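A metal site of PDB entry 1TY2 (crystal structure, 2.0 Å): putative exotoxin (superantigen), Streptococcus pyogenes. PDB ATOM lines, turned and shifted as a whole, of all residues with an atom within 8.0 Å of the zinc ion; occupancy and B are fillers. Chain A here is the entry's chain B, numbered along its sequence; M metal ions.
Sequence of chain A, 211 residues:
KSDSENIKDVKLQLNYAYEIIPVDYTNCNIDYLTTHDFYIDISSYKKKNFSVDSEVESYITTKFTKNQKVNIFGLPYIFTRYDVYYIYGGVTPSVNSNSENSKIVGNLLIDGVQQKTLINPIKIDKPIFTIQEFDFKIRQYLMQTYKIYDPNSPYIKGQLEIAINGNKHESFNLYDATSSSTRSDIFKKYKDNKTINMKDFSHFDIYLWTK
OD2 of Asp 205 is bound to the zinc ion (2.0 Å). NE2 of His 203 binds the zinc ion (2.3 Å). The zinc ion is bound by NE2 of His 169, at 2.5 Å. The zinc ion has three donor atoms within binding distance.
Within 4 Å of the zinc ion: His 169, His 203 and Asp 205. The nearest printed residue that does not touch the zinc ion is Ala 163 (4.6 Å).
The backbone NH (N) of Glu 161 lies within hydrogen-bond range of the backbone carbonyl oxygen (O) of Asp 205. The side-chain amide nitrogen (ND2) of Asn 107 sits at hydrogen-bond distance from the side-chain carboxylate (OD1) of Asp 205. The backbone NH (N) of Ala 163 lies within hydrogen-bond range of the backbone carbonyl oxygen (O) of His 203 (2.9 Å). A ring nitrogen (ND1) of His 203 lies within hydrogen-bond range of the side-chain hydroxyl of Ser 202 (3.0 Å).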
ATOM      1  N   GLY A 106      -1.544  10.098   5.458  1.00  0.00           N
ATOM      2  CA  GLY A 106      -2.483  11.014   4.850  1.00  0.00           C
ATOM      3  C   GLY A 106      -1.868  12.382   4.666  1.00  0.00           C
ATOM      4  O   GLY A 106      -0.673  12.560   4.884  1.00  0.00           O
ATOM      5  N   ASN A 107      -2.682  13.344   4.262  1.00  0.00           N
ATOM      6  CA  ASN A 107      -2.191  14.699   4.057  1.00  0.00           C
ATOM      7  C   ASN A 107      -3.066  15.719   4.762  1.00  0.00           C
ATOM      8  O   ASN A 107      -4.202  15.416   5.148  1.00  0.00           O
ATOM      9  CB  ASN A 107      -2.149  14.994   2.558  1.00  0.00           C
ATOM     10  CG  ASN A 107      -1.536  13.864   1.772  1.00  0.00           C
ATOM     11  OD1 ASN A 107      -0.351  13.543   1.928  1.00  0.00           O
ATOM     12  ND2 ASN A 107      -2.348  13.228   0.921  1.00  0.00           N
ATOM     13  N   GLU A 161     -11.332  13.276   5.692  1.00  0.00           N
ATOM     14  CA  GLU A 161     -11.728  12.350   4.639  1.00  0.00           C
ATOM     15  C   GLU A 161     -10.980  11.037   4.825  1.00  0.00           C
ATOM     16  O   GLU A 161      -9.781  11.036   5.081  1.00  0.00           O
ATOM     17  CB  GLU A 161     -11.418  12.944   3.269  1.00  0.00           C
ATOM     18  N   ILE A 162     -11.694   9.936   4.700  1.00  0.00           N
ATOM     19  CA  ILE A 162     -11.095   8.623   4.855  1.00  0.00           C
ATOM     20  C   ILE A 162     -11.264   7.832   3.572  1.00  0.00           C
ATOM     21  O   ILE A 162     -12.393   7.533   3.161  1.00  0.00           O
ATOM     22  CB  ILE A 162     -11.750   7.858   6.024  1.00  0.00           C
ATOM     23  CG1 ILE A 162     -11.463   8.591   7.337  1.00  0.00           C
ATOM     24  CG2 ILE A 162     -11.212   6.426   6.071  1.00  0.00           C
ATOM     25  CD1 ILE A 162     -12.112   7.962   8.550  1.00  0.00           C
ATOM     26  N   ALA A 163     -10.149   7.493   2.931  1.00  0.00           N
ATOM     27  CA  ALA A 163     -10.176   6.716   1.677  1.00  0.00           C
ATOM     28  C   ALA A 163     -10.015   5.227   1.963  1.00  0.00           C
ATOM     29  O   ALA A 163      -9.075   4.806   2.631  1.00  0.00           O
ATOM     30  CB  ALA A 163      -9.058   7.190   0.754  1.00  0.00           C
ATOM     31  N   ILE A 164     -10.948   4.438   1.448  1.00  0.00           N
ATOM     32  CA  ILE A 164     -10.957   2.988   1.634  1.00  0.00           C
ATOM     33  C   ILE A 164     -10.813   2.263   0.305  1.00  0.00           C
ATOM     34  O   ILE A 164     -11.616   2.480  -0.602  1.00  0.00           O
ATOM     35  CB  ILE A 164     -12.277   2.540   2.299  1.00  0.00           C
ATOM     36  CG1 ILE A 164     -12.297   3.012   3.748  1.00  0.00           C
ATOM     37  CG2 ILE A 164     -12.430   1.035   2.186  1.00  0.00           C
ATOM     38  CD1 ILE A 164     -13.599   2.750   4.455  1.00  0.00           C
ATOM     39  N   HIS A 169     -14.715   7.818  -1.041  1.00  0.00           N
ATOM     40  CA  HIS A 169     -14.232   8.494   0.155  1.00  0.00           C
ATOM     41  C   HIS A 169     -15.386   8.666   1.128  1.00  0.00           C
ATOM     42  O   HIS A 169     -16.564   8.535   0.759  1.00  0.00           O
ATOM     43  CB  HIS A 169     -13.689   9.888  -0.189  1.00  0.00           C
ATOM     44  CG  HIS A 169     -12.235   9.911  -0.575  1.00  0.00           C
ATOM     45  ND1 HIS A 169     -11.692   9.074  -1.526  1.00  0.00           N
ATOM     46  CD2 HIS A 169     -11.224  10.721  -0.167  1.00  0.00           C
ATOM     47  CE1 HIS A 169     -10.421   9.367  -1.690  1.00  0.00           C
ATOM     48  NE2 HIS A 169     -10.105  10.361  -0.877  1.00  0.00           N
ATOM     49  N   SER A 202      -6.673   3.085   2.846  1.00  0.00           N
ATOM     50  CA  SER A 202      -5.786   3.666   1.841  1.00  0.00           C
ATOM     51  C   SER A 202      -5.009   4.823   2.454  1.00  0.00           C
ATOM     52  O   SER A 202      -3.794   4.750   2.609  1.00  0.00           O
ATOM     53  CB  SER A 202      -6.600   4.164   0.641  1.00  0.00           C
ATOM     54  OG  SER A 202      -5.754   4.804  -0.293  1.00  0.00           O
ATOM     55  N   HIS A 203      -5.719   5.889   2.805  1.00  0.00           N
ATOM     56  CA  HIS A 203      -5.099   7.065   3.393  1.00  0.00           C
ATOM     57  C   HIS A 203      -6.204   8.010   3.869  1.00  0.00           C
ATOM     58  O   HIS A 203      -7.387   7.695   3.759  1.00  0.00           O
ATOM     59  CB  HIS A 203      -4.242   7.784   2.349  1.00  0.00           C
ATOM     60  CG  HIS A 203      -5.062   8.434   1.262  1.00  0.00           C
ATOM     61  ND1 HIS A 203      -5.687   7.713   0.273  1.00  0.00           N
ATOM     62  CD2 HIS A 203      -5.389   9.727   1.054  1.00  0.00           C
ATOM     63  CE1 HIS A 203      -6.367   8.533  -0.500  1.00  0.00           C
ATOM     64  NE2 HIS A 203      -6.199   9.762  -0.051  1.00  0.00           N
ATOM     65  N   PHE A 204      -5.809   9.168   4.390  1.00  0.00           N
ATOM     66  CA  PHE A 204      -6.776  10.151   4.852  1.00  0.00           C
ATOM     67  C   PHE A 204      -6.356  11.536   4.359  1.00  0.00           C
ATOM     68  O   PHE A 204      -5.198  11.751   4.001  1.00  0.00           O
ATOM     69  CB  PHE A 204      -6.859  10.165   6.388  1.00  0.00           C
ATOM     70  CG  PHE A 204      -5.590  10.620   7.063  1.00  0.00           C
ATOM     71  CD1 PHE A 204      -5.291  11.977   7.179  1.00  0.00           C
ATOM     72  CD2 PHE A 204      -4.682   9.698   7.568  1.00  0.00           C
ATOM     73  CE1 PHE A 204      -4.110  12.398   7.782  1.00  0.00           C
ATOM     74  CE2 PHE A 204      -3.487  10.110   8.174  1.00  0.00           C
ATOM     75  CZ  PHE A 204      -3.205  11.458   8.273  1.00  0.00           C
ATOM     76  N   ASP A 205      -7.308  12.456   4.334  1.00  0.00           N
ATOM     77  CA  ASP A 205      -7.025  13.835   3.947  1.00  0.00           C
ATOM     78  C   ASP A 205      -7.706  14.760   4.950  1.00  0.00           C
ATOM     79  O   ASP A 205      -8.925  14.675   5.166  1.00  0.00           O
ATOM     80  CB  ASP A 205      -7.550  14.120   2.535  1.00  0.00           C
ATOM     81  CG  ASP A 205      -6.793  13.341   1.476  1.00  0.00           C
ATOM     82  OD1 ASP A 205      -5.561  13.503   1.372  1.00  0.00           O
ATOM     83  OD2 ASP A 205      -7.440  12.561   0.744  1.00  0.00           O
ATOM     84  N   ILE A 206      -6.917  15.611   5.587  1.00  0.00           N
ATOM     85  CA  ILE A 206      -7.435  16.567   6.564  1.00  0.00           C
ATOM     86  C   ILE A 206      -7.508  17.931   5.882  1.00  0.00           C
ATOM     87  O   ILE A 206      -6.507  18.417   5.336  1.00  0.00           O
ATOM     88  CB  ILE A 206      -6.515  16.687   7.794  1.00  0.00           C
ATOM     89  CG1 ILE A 206      -6.425  15.350   8.534  1.00  0.00           C
ATOM     90  CG2 ILE A 206      -7.021  17.788   8.715  1.00  0.00           C
ATOM     91  CD1 ILE A 206      -7.710  14.929   9.173  1.00  0.00           C
ATOM     92  N   TYR A 207      -8.684  18.562   5.910  1.00  0.00           N
ATOM     93  CA  TYR A 207      -8.852  19.873   5.312  1.00  0.00           C
ATOM     94  C   TYR A 207      -9.313  20.854   6.386  1.00  0.00           C
ATOM     95  O   TYR A 207     -10.346  20.638   7.029  1.00  0.00           O
ATOM     96  CB  TYR A 207      -9.912  19.833   4.204  1.00  0.00           C
ATOM     97  CG  TYR A 207      -9.659  18.836   3.100  1.00  0.00           C
ATOM     98  CD1 TYR A 207      -8.812  19.129   2.027  1.00  0.00           C
ATOM     99  CD2 TYR A 207     -10.284  17.586   3.121  1.00  0.00           C
ATOM    100  CE1 TYR A 207      -8.605  18.205   0.992  1.00  0.00           C
ATOM    101  CE2 TYR A 207     -10.087  16.659   2.100  1.00  0.00           C
ATOM    102  CZ  TYR A 207      -9.247  16.965   1.039  1.00  0.00           C
ATOM    103  OH  TYR A 207      -9.071  16.032   0.030  1.00  0.00           O
HETATM  104 ZN    ZN M   1      -7.739  11.280  -0.750  1.00  0.00          ZN
